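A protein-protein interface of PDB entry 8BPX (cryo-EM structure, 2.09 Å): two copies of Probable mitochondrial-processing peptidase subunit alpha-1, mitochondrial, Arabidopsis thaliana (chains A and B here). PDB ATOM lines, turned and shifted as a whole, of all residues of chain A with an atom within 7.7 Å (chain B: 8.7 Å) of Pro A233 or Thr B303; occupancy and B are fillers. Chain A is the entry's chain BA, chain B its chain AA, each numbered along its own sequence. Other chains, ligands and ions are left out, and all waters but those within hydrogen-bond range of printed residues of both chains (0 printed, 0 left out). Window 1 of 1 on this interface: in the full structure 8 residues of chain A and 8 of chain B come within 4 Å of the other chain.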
ATOM      1  N   HIS A 117     -14.150  18.230 -10.883  1.00  0.00           N
ATOM      2  CA  HIS A 117     -15.175  17.861  -9.913  1.00  0.00           C
ATOM      3  C   HIS A 117     -14.968  16.428  -9.435  1.00  0.00           C
ATOM      4  O   HIS A 117     -15.007  15.485 -10.230  1.00  0.00           O
ATOM      5  CB  HIS A 117     -16.565  18.036 -10.520  1.00  0.00           C
ATOM      6  CG  HIS A 117     -17.077  19.439 -10.439  1.00  0.00           C
ATOM      7  ND1 HIS A 117     -17.835  20.015 -11.435  1.00  0.00           N
ATOM      8  CD2 HIS A 117     -16.911  20.394  -9.494  1.00  0.00           C
ATOM      9  CE1 HIS A 117     -18.128  21.257 -11.099  1.00  0.00           C
ATOM     10  NE2 HIS A 117     -17.578  21.513  -9.925  1.00  0.00           N
ATOM     11  N   GLY A 118     -14.761  16.270  -8.128  1.00  0.00           N
ATOM     12  CA  GLY A 118     -14.443  14.990  -7.537  1.00  0.00           C
ATOM     13  C   GLY A 118     -12.975  14.755  -7.275  1.00  0.00           C
ATOM     14  O   GLY A 118     -12.623  13.699  -6.740  1.00  0.00           O
ATOM     15  N   MET A 198     -14.473   4.183  -4.737  1.00  0.00           N
ATOM     16  CA  MET A 198     -15.242   5.411  -4.587  1.00  0.00           C
ATOM     17  C   MET A 198     -16.684   5.213  -5.030  1.00  0.00           C
ATOM     18  O   MET A 198     -17.604   5.800  -4.452  1.00  0.00           O
ATOM     19  CB  MET A 198     -14.587   6.534  -5.390  1.00  0.00           C
ATOM     20  CG  MET A 198     -13.851   7.557  -4.557  1.00  0.00           C
ATOM     21  SD  MET A 198     -12.960   8.757  -5.559  1.00  0.00           S
ATOM     22  CE  MET A 198     -14.286   9.831  -6.085  1.00  0.00           C
ATOM     23  N   LYS A 199     -16.895   4.408  -6.075  1.00  0.00           N
ATOM     24  CA  LYS A 199     -18.257   4.121  -6.522  1.00  0.00           C
ATOM     25  C   LYS A 199     -19.097   3.547  -5.386  1.00  0.00           C
ATOM     26  O   LYS A 199     -20.199   4.032  -5.098  1.00  0.00           O
ATOM     27  CB  LYS A 199     -18.239   3.144  -7.698  1.00  0.00           C
ATOM     28  CG  LYS A 199     -17.482   3.611  -8.922  1.00  0.00           C
ATOM     29  CD  LYS A 199     -18.148   4.792  -9.586  1.00  0.00           C
ATOM     30  CE  LYS A 199     -17.259   5.362 -10.670  1.00  0.00           C
ATOM     31  NZ  LYS A 199     -15.889   4.780 -10.631  1.00  0.00           N
ATOM     32  N   ILE A 202     -19.773   6.065  -2.568  1.00  0.00           N
ATOM     33  CA  ILE A 202     -20.858   6.969  -2.937  1.00  0.00           C
ATOM     34  C   ILE A 202     -22.203   6.268  -2.811  1.00  0.00           C
ATOM     35  O   ILE A 202     -23.171   6.837  -2.292  1.00  0.00           O
ATOM     36  CB  ILE A 202     -20.635   7.508  -4.361  1.00  0.00           C
ATOM     37  CG1 ILE A 202     -19.616   8.645  -4.351  1.00  0.00           C
ATOM     38  CG2 ILE A 202     -21.950   7.958  -4.980  1.00  0.00           C
ATOM     39  CD1 ILE A 202     -20.201   9.985  -3.993  1.00  0.00           C
ATOM     40  N   PRO A 229     -20.040  19.802  -4.688  1.00  0.00           N
ATOM     41  CA  PRO A 229     -20.087  18.646  -3.785  1.00  0.00           C
ATOM     42  C   PRO A 229     -18.696  18.164  -3.402  1.00  0.00           C
ATOM     43  O   PRO A 229     -17.776  18.145  -4.221  1.00  0.00           O
ATOM     44  CB  PRO A 229     -20.841  17.589  -4.602  1.00  0.00           C
ATOM     45  CG  PRO A 229     -20.782  18.061  -6.017  1.00  0.00           C
ATOM     46  CD  PRO A 229     -20.729  19.546  -5.962  1.00  0.00           C
ATOM     47  N   LEU A 230     -18.553  17.775  -2.134  1.00  0.00           N
ATOM     48  CA  LEU A 230     -17.392  16.992  -1.729  1.00  0.00           C
ATOM     49  C   LEU A 230     -17.485  15.576  -2.284  1.00  0.00           C
ATOM     50  O   LEU A 230     -16.469  14.971  -2.644  1.00  0.00           O
ATOM     51  CB  LEU A 230     -17.283  16.974  -0.205  1.00  0.00           C
ATOM     52  CG  LEU A 230     -15.933  16.778   0.475  1.00  0.00           C
ATOM     53  CD1 LEU A 230     -14.833  17.551  -0.237  1.00  0.00           C
ATOM     54  CD2 LEU A 230     -16.042  17.212   1.926  1.00  0.00           C
ATOM     55  N   TYR A 231     -18.700  15.038  -2.365  1.00  0.00           N
ATOM     56  CA  TYR A 231     -18.969  13.737  -2.967  1.00  0.00           C
ATOM     57  C   TYR A 231     -19.450  13.966  -4.395  1.00  0.00           C
ATOM     58  O   TYR A 231     -20.585  14.404  -4.611  1.00  0.00           O
ATOM     59  CB  TYR A 231     -20.016  12.973  -2.162  1.00  0.00           C
ATOM     60  CG  TYR A 231     -19.542  12.455  -0.826  1.00  0.00           C
ATOM     61  CD1 TYR A 231     -19.437  13.299   0.269  1.00  0.00           C
ATOM     62  CD2 TYR A 231     -19.222  11.117  -0.654  1.00  0.00           C
ATOM     63  CE1 TYR A 231     -19.012  12.830   1.487  1.00  0.00           C
ATOM     64  CE2 TYR A 231     -18.799  10.638   0.566  1.00  0.00           C
ATOM     65  CZ  TYR A 231     -18.694  11.499   1.633  1.00  0.00           C
ATOM     66  OH  TYR A 231     -18.269  11.027   2.855  1.00  0.00           O
ATOM     67  N   ALA A 232     -18.598  13.665  -5.366  1.00  0.00           N
ATOM     68  CA  ALA A 232     -18.952  13.904  -6.755  1.00  0.00           C
ATOM     69  C   ALA A 232     -19.923  12.839  -7.261  1.00  0.00           C
ATOM     70  O   ALA A 232     -19.931  11.710  -6.764  1.00  0.00           O
ATOM     71  CB  ALA A 232     -17.706  13.914  -7.628  1.00  0.00           C
ATOM     72  N   PRO A 233     -20.747  13.172  -8.251  1.00  0.00           N
ATOM     73  CA  PRO A 233     -21.669  12.180  -8.809  1.00  0.00           C
ATOM     74  C   PRO A 233     -20.933  11.147  -9.646  1.00  0.00           C
ATOM     75  O   PRO A 233     -19.795  11.348 -10.077  1.00  0.00           O
ATOM     76  CB  PRO A 233     -22.613  13.019  -9.673  1.00  0.00           C
ATOM     77  CG  PRO A 233     -21.806  14.196 -10.063  1.00  0.00           C
ATOM     78  CD  PRO A 233     -20.845  14.469  -8.944  1.00  0.00           C
ATOM     79  N   GLU A 234     -21.611  10.026  -9.889  1.00  0.00           N
ATOM     80  CA  GLU A 234     -20.997   8.935 -10.632  1.00  0.00           C
ATOM     81  C   GLU A 234     -21.081   9.196 -12.129  1.00  0.00           C
ATOM     82  O   GLU A 234     -21.449   8.312 -12.910  1.00  0.00           O
ATOM     83  CB  GLU A 234     -21.667   7.602 -10.279  1.00  0.00           C
ATOM     84  CG  GLU A 234     -23.188   7.590 -10.440  1.00  0.00           C
ATOM     85  CD  GLU A 234     -23.917   8.175  -9.245  1.00  0.00           C
ATOM     86  OE1 GLU A 234     -23.800   9.397  -9.015  1.00  0.00           O
ATOM     87  OE2 GLU A 234     -24.611   7.414  -8.538  1.00  0.00           O
ATOM     88  N   SER A 235     -20.736  10.401 -12.527  1.00  0.00           N
ATOM     89  CA  SER A 235     -20.498  10.815 -13.902  1.00  0.00           C
ATOM     90  C   SER A 235     -19.184  11.563 -14.045  1.00  0.00           C
ATOM     91  O   SER A 235     -18.494  11.401 -15.053  1.00  0.00           O
ATOM     92  CB  SER A 235     -21.658  11.688 -14.404  1.00  0.00           C
ATOM     93  OG  SER A 235     -21.222  12.562 -15.428  1.00  0.00           O
ATOM     94  N   ALA A 236     -18.819  12.373 -13.050  1.00  0.00           N
ATOM     95  CA  ALA A 236     -17.497  12.979 -13.013  1.00  0.00           C
ATOM     96  C   ALA A 236     -16.416  11.973 -12.650  1.00  0.00           C
ATOM     97  O   ALA A 236     -15.231  12.269 -12.822  1.00  0.00           O
ATOM     98  CB  ALA A 236     -17.477  14.143 -12.022  1.00  0.00           C
ATOM     99  N   LEU A 237     -16.801  10.800 -12.139  1.00  0.00           N
ATOM    100  CA  LEU A 237     -15.826   9.775 -11.787  1.00  0.00           C
ATOM    101  C   LEU A 237     -15.306   9.037 -13.011  1.00  0.00           C
ATOM    102  O   LEU A 237     -14.119   8.694 -13.062  1.00  0.00           O
ATOM    103  CB  LEU A 237     -16.443   8.782 -10.800  1.00  0.00           C
ATOM    104  CG  LEU A 237     -17.083   9.393  -9.552  1.00  0.00           C
ATOM    105  CD1 LEU A 237     -17.389   8.321  -8.521  1.00  0.00           C
ATOM    106  CD2 LEU A 237     -16.190  10.473  -8.968  1.00  0.00           C
ATOM    107  N   ASP A 238     -16.167   8.791 -14.001  1.00  0.00           N
ATOM    108  CA  ASP A 238     -15.739   8.143 -15.235  1.00  0.00           C
ATOM    109  C   ASP A 238     -14.728   8.978 -16.007  1.00  0.00           C
ATOM    110  O   ASP A 238     -14.056   8.444 -16.895  1.00  0.00           O
ATOM    111  CB  ASP A 238     -16.953   7.851 -16.119  1.00  0.00           C
ATOM    112  CG  ASP A 238     -17.821   6.735 -15.571  1.00  0.00           C
ATOM    113  OD1 ASP A 238     -17.869   6.569 -14.333  1.00  0.00           O
ATOM    114  OD2 ASP A 238     -18.461   6.028 -16.376  1.00  0.00           O
ATOM    115  N   LEU A 240     -12.430  11.102 -14.217  1.00  0.00           N
ATOM    116  CA  LEU A 240     -11.261  11.312 -13.378  1.00  0.00           C
ATOM    117  C   LEU A 240     -10.163  10.315 -13.735  1.00  0.00           C
ATOM    118  O   LEU A 240     -10.434   9.139 -13.989  1.00  0.00           O
ATOM    119  CB  LEU A 240     -11.650  11.184 -11.905  1.00  0.00           C
ATOM    120  CG  LEU A 240     -12.168  12.461 -11.231  1.00  0.00           C
ATOM    121  CD1 LEU A 240     -12.679  12.163  -9.833  1.00  0.00           C
ATOM    122  CD2 LEU A 240     -11.083  13.523 -11.184  1.00  0.00           C
ATOM    123  N   ALA B 206     -35.438   7.955 -17.287  1.00  0.00           N
ATOM    124  CA  ALA B 206     -34.403   8.974 -17.400  1.00  0.00           C
ATOM    125  C   ALA B 206     -33.944   9.174 -18.837  1.00  0.00           C
ATOM    126  O   ALA B 206     -33.248  10.153 -19.125  1.00  0.00           O
ATOM    127  CB  ALA B 206     -33.212   8.610 -16.514  1.00  0.00           C
ATOM    128  N   PHE B 212     -39.595  12.984 -18.285  1.00  0.00           N
ATOM    129  CA  PHE B 212     -39.092  13.042 -16.918  1.00  0.00           C
ATOM    130  C   PHE B 212     -39.325  14.417 -16.308  1.00  0.00           C
ATOM    131  O   PHE B 212     -39.838  14.534 -15.188  1.00  0.00           O
ATOM    132  CB  PHE B 212     -37.606  12.687 -16.901  1.00  0.00           C
ATOM    133  CG  PHE B 212     -37.054  12.453 -15.531  1.00  0.00           C
ATOM    134  CD1 PHE B 212     -37.186  11.222 -14.915  1.00  0.00           C
ATOM    135  CD2 PHE B 212     -36.400  13.467 -14.854  1.00  0.00           C
ATOM    136  CE1 PHE B 212     -36.679  11.011 -13.652  1.00  0.00           C
ATOM    137  CE2 PHE B 212     -35.894  13.260 -13.594  1.00  0.00           C
ATOM    138  CZ  PHE B 212     -36.032  12.030 -12.992  1.00  0.00           C
ATOM    139  N   PHE B 299     -37.401  21.535  -9.138  1.00  0.00           N
ATOM    140  CA  PHE B 299     -36.961  20.148  -9.186  1.00  0.00           C
ATOM    141  C   PHE B 299     -35.528  20.113  -9.682  1.00  0.00           C
ATOM    142  O   PHE B 299     -35.223  20.674 -10.740  1.00  0.00           O
ATOM    143  CB  PHE B 299     -37.838  19.309 -10.111  1.00  0.00           C
ATOM    144  CG  PHE B 299     -37.244  17.974 -10.443  1.00  0.00           C
ATOM    145  CD1 PHE B 299     -37.226  16.961  -9.504  1.00  0.00           C
ATOM    146  CD2 PHE B 299     -36.664  17.747 -11.680  1.00  0.00           C
ATOM    147  CE1 PHE B 299     -36.676  15.736  -9.804  1.00  0.00           C
ATOM    148  CE2 PHE B 299     -36.111  16.529 -11.984  1.00  0.00           C
ATOM    149  CZ  PHE B 299     -36.116  15.519 -11.044  1.00  0.00           C
ATOM    150  N   ARG B 300     -34.655  19.436  -8.940  1.00  0.00           N
ATOM    151  CA  ARG B 300     -33.230  19.462  -9.254  1.00  0.00           C
ATOM    152  C   ARG B 300     -32.608  18.120  -8.918  1.00  0.00           C
ATOM    153  O   ARG B 300     -32.549  17.734  -7.746  1.00  0.00           O
ATOM    154  CB  ARG B 300     -32.530  20.583  -8.495  1.00  0.00           C
ATOM    155  CG  ARG B 300     -32.793  21.922  -9.110  1.00  0.00           C
ATOM    156  CD  ARG B 300     -31.918  23.022  -8.590  1.00  0.00           C
ATOM    157  NE  ARG B 300     -32.262  24.247  -9.295  1.00  0.00           N
ATOM    158  CZ  ARG B 300     -31.765  25.444  -9.027  1.00  0.00           C
ATOM    159  NH1 ARG B 300     -30.893  25.629  -8.050  1.00  0.00           N
ATOM    160  NH2 ARG B 300     -32.157  26.482  -9.757  1.00  0.00           N
ATOM    161  N   GLN B 301     -32.149  17.416  -9.943  1.00  0.00           N
ATOM    162  CA  GLN B 301     -31.355  16.209  -9.781  1.00  0.00           C
ATOM    163  C   GLN B 301     -30.030  16.433 -10.495  1.00  0.00           C
ATOM    164  O   GLN B 301     -29.944  16.275 -11.716  1.00  0.00           O
ATOM    165  CB  GLN B 301     -32.080  14.986 -10.332  1.00  0.00           C
ATOM    166  CG  GLN B 301     -32.742  14.134  -9.268  1.00  0.00           C
ATOM    167  CD  GLN B 301     -33.346  12.871  -9.840  1.00  0.00           C
ATOM    168  OE1 GLN B 301     -32.832  12.306 -10.804  1.00  0.00           O
ATOM    169  NE2 GLN B 301     -34.447  12.420  -9.248  1.00  0.00           N
ATOM    170  N   HIS B 302     -29.007  16.804  -9.734  1.00  0.00           N
ATOM    171  CA  HIS B 302     -27.672  17.008 -10.284  1.00  0.00           C
ATOM    172  C   HIS B 302     -27.055  15.645 -10.556  1.00  0.00           C
ATOM    173  O   HIS B 302     -26.572  14.969  -9.644  1.00  0.00           O
ATOM    174  CB  HIS B 302     -26.812  17.830  -9.333  1.00  0.00           C
ATOM    175  CG  HIS B 302     -25.343  17.662  -9.554  1.00  0.00           C
ATOM    176  ND1 HIS B 302     -24.489  17.216  -8.570  1.00  0.00           N
ATOM    177  CD2 HIS B 302     -24.579  17.861 -10.654  1.00  0.00           C
ATOM    178  CE1 HIS B 302     -23.259  17.160  -9.049  1.00  0.00           C
ATOM    179  NE2 HIS B 302     -23.288  17.542 -10.313  1.00  0.00           N
ATOM    180  N   THR B 303     -27.094  15.226 -11.817  1.00  0.00           N
ATOM    181  CA  THR B 303     -26.450  13.988 -12.227  1.00  0.00           C
ATOM    182  C   THR B 303     -25.054  14.214 -12.784  1.00  0.00           C
ATOM    183  O   THR B 303     -24.251  13.274 -12.809  1.00  0.00           O
ATOM    184  CB  THR B 303     -27.303  13.268 -13.273  1.00  0.00           C
ATOM    185  OG1 THR B 303     -28.579  12.944 -12.710  1.00  0.00           O
ATOM    186  CG2 THR B 303     -26.618  11.987 -13.724  1.00  0.00           C
ATOM    187  N   GLY B 304     -24.750  15.431 -13.227  1.00  0.00           N
ATOM    188  CA  GLY B 304     -23.447  15.735 -13.774  1.00  0.00           C
ATOM    189  C   GLY B 304     -23.299  15.248 -15.201  1.00  0.00           C
ATOM    190  O   GLY B 304     -24.162  14.575 -15.767  1.00  0.00           O
ATOM    191  N   GLY B 305     -22.164  15.606 -15.793  1.00  0.00           N
ATOM    192  CA  GLY B 305     -21.852  15.172 -17.139  1.00  0.00           C
ATOM    193  C   GLY B 305     -22.066  16.233 -18.195  1.00  0.00           C
ATOM    194  O   GLY B 305     -21.282  17.180 -18.307  1.00  0.00           O
ATOM    195  N   GLU B 306     -23.130  16.086 -18.978  1.00  0.00           N
ATOM    196  CA  GLU B 306     -23.368  16.944 -20.130  1.00  0.00           C
ATOM    197  C   GLU B 306     -24.861  16.960 -20.419  1.00  0.00           C
ATOM    198  O   GLU B 306     -25.646  16.262 -19.769  1.00  0.00           O
ATOM    199  CB  GLU B 306     -22.571  16.452 -21.343  1.00  0.00           C
ATOM    200  CG  GLU B 306     -23.253  15.344 -22.154  1.00  0.00           C
ATOM    201  CD  GLU B 306     -23.304  13.989 -21.449  1.00  0.00           C
ATOM    202  OE1 GLU B 306     -23.294  13.938 -20.200  1.00  0.00           O
ATOM    203  OE2 GLU B 306     -23.364  12.964 -22.157  1.00  0.00           O
ATOM    204  N   ALA B 307     -25.249  17.770 -21.406  1.00  0.00           N
ATOM    205  CA  ALA B 307     -26.603  17.782 -21.955  1.00  0.00           C
ATOM    206  C   ALA B 307     -27.639  18.077 -20.867  1.00  0.00           C
ATOM    207  O   ALA B 307     -28.456  17.233 -20.493  1.00  0.00           O
ATOM    208  CB  ALA B 307     -26.910  16.462 -22.672  1.00  0.00           C
ATOM    209  N   SER B 485     -35.075  21.227 -13.671  1.00  0.00           N
ATOM    210  CA  SER B 485     -33.862  20.989 -14.439  1.00  0.00           C
ATOM    211  C   SER B 485     -33.365  19.577 -14.165  1.00  0.00           C
ATOM    212  O   SER B 485     -33.614  19.012 -13.098  1.00  0.00           O
ATOM    213  CB  SER B 485     -32.768  22.014 -14.105  1.00  0.00           C
ATOM    214  OG  SER B 485     -32.854  22.435 -12.755  1.00  0.00           O
ATOM    215  N   PHE B 486     -32.659  19.016 -15.142  1.00  0.00           N
ATOM    216  CA  PHE B 486     -32.249  17.616 -15.086  1.00  0.00           C
ATOM    217  C   PHE B 486     -30.967  17.454 -15.887  1.00  0.00           C
ATOM    218  O   PHE B 486     -30.940  17.744 -17.086  1.00  0.00           O
ATOM    219  CB  PHE B 486     -33.359  16.710 -15.629  1.00  0.00           C
ATOM    220  CG  PHE B 486     -32.908  15.317 -15.969  1.00  0.00           C
ATOM    221  CD1 PHE B 486     -32.190  14.561 -15.059  1.00  0.00           C
ATOM    222  CD2 PHE B 486     -33.213  14.764 -17.197  1.00  0.00           C
ATOM    223  CE1 PHE B 486     -31.778  13.279 -15.374  1.00  0.00           C
ATOM    224  CE2 PHE B 486     -32.805  13.483 -17.520  1.00  0.00           C
ATOM    225  CZ  PHE B 486     -32.086  12.739 -16.607  1.00  0.00           C
ATOM    226  N   GLY B 487     -29.916  16.983 -15.226  1.00  0.00           N
ATOM    227  CA  GLY B 487     -28.619  16.841 -15.856  1.00  0.00           C
ATOM    228  C   GLY B 487     -27.521  17.425 -14.994  1.00  0.00           C
ATOM    229  O   GLY B 487     -27.326  17.001 -13.852  1.00  0.00           O
ATOM    230  N   ASP B 488     -26.792  18.398 -15.531  1.00  0.00           N
ATOM    231  CA  ASP B 488     -25.809  19.155 -14.764  1.00  0.00           C
ATOM    232  C   ASP B 488     -26.482  20.452 -14.335  1.00  0.00           C
ATOM    233  O   ASP B 488     -26.678  21.361 -15.145  1.00  0.00           O
ATOM    234  CB  ASP B 488     -24.548  19.415 -15.579  1.00  0.00           C
ATOM    235  CG  ASP B 488     -23.504  20.192 -14.803  1.00  0.00           C
ATOM    236  OD1 ASP B 488     -22.983  19.654 -13.804  1.00  0.00           O
ATOM    237  OD2 ASP B 488     -23.211  21.343 -15.186  1.00  0.00           O
ATOM    238  N   VAL B 489     -26.836  20.534 -13.051  1.00  0.00           N
ATOM    239  CA  VAL B 489     -27.591  21.670 -12.534  1.00  0.00           C
ATOM    240  C   VAL B 489     -26.701  22.668 -11.796  1.00  0.00           C
ATOM    241  O   VAL B 489     -27.184  23.740 -11.396  1.00  0.00           O
ATOM    242  CB  VAL B 489     -28.747  21.174 -11.632  1.00  0.00           C
ATOM    243  CG1 VAL B 489     -29.698  22.300 -11.247  1.00  0.00           C
ATOM    244  CG2 VAL B 489     -29.512  20.056 -12.325  1.00  0.00           C
ATOM    245  N   LEU B 490     -25.406  22.373 -11.641  1.00  0.00           N
ATOM    246  CA  LEU B 490     -24.529  23.262 -10.884  1.00  0.00           C
ATOM    247  C   LEU B 490     -24.465  24.649 -11.506  1.00  0.00           C
ATOM    248  O   LEU B 490     -24.537  25.659 -10.799  1.00  0.00           O
ATOM    249  CB  LEU B 490     -23.125  22.666 -10.789  1.00  0.00           C
ATOM    250  CG  LEU B 490     -22.894  21.515  -9.812  1.00  0.00           C
ATOM    251  CD1 LEU B 490     -22.008  20.470 -10.455  1.00  0.00           C
ATOM    252  CD2 LEU B 490     -22.280  22.023  -8.518  1.00  0.00           C
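The side-chain hydroxyl (OG) of Ser A235 lies close to the backbone NH (N) of Gly B305.
The backbone NH (N) of Thr B303 lies within hydrogen-bond range of the backbone carbonyl oxygen (O) of Gly B487 (2.7 Å). The backbone carbonyl oxygen (O) of Gly B487 sits at hydrogen-bond distance from the backbone NH (N) of Gly B304 (3.1 Å).
Among the printed residues, pairs that only touch across the chains: Ser A235 with Gly B304, Ser A235 with Thr B303, Pro A233 with His B302, Pro A233 with Thr B303 and Pro A229 with Leu B490.
Of the printed residues of chain B, Pro A229 touches Leu B490 (3.9 Å). Pro A233 touches just these residues of chain B: His B302 and Thr B303. Glu A234 touches none of the printed residues of chain B. Printed residues of chain B within 4 Å of Ser A235: Thr B303 (3.4 Å), Gly B304 (3.4 Å) and Gly B305 (3.2 Å). Of the printed residues of chain A, His B302 touches Pro A233 (3.5 Å). Thr B303 touches just these residues of chain A: Pro A233 (3.5 Å) and Ser A235 (3.4 Å). Of chain A, only Ser A235 comes within 4 Å of Gly B304. Of the printed residues of chain A, Gly B305 touches Ser A235 (3.2 Å). Val B489 touches none of the printed residues of chain A. Printed residues of chain A within 4 Å of Leu B490: Pro A229 (3.9 Å). The nearest residue of chain A that does not touch Thr B303 is Glu A234 (5.1 Å). The nearest printed residue of chain A that does not touch Leu B490 is His A117 (4.01 Å).
Of the 16 printed residues of chain A, 3 touch a printed residue of chain B. Printed residues of chain A that touch a printed residue of chain B: Pro A229, Pro A233 and Ser A235. Printed residues of chain B that touch a printed residue of chain A: His B302, Thr B303, Gly B304, Gly B305 and Leu B490. Among the printed residues, 6 pairs touch across the chains. Among the printed residues, no Asp or Glu carboxylate lies within 4 Å of a Lys or Arg side-chain nitrogen of the other chain.
No position is printed for both chains.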
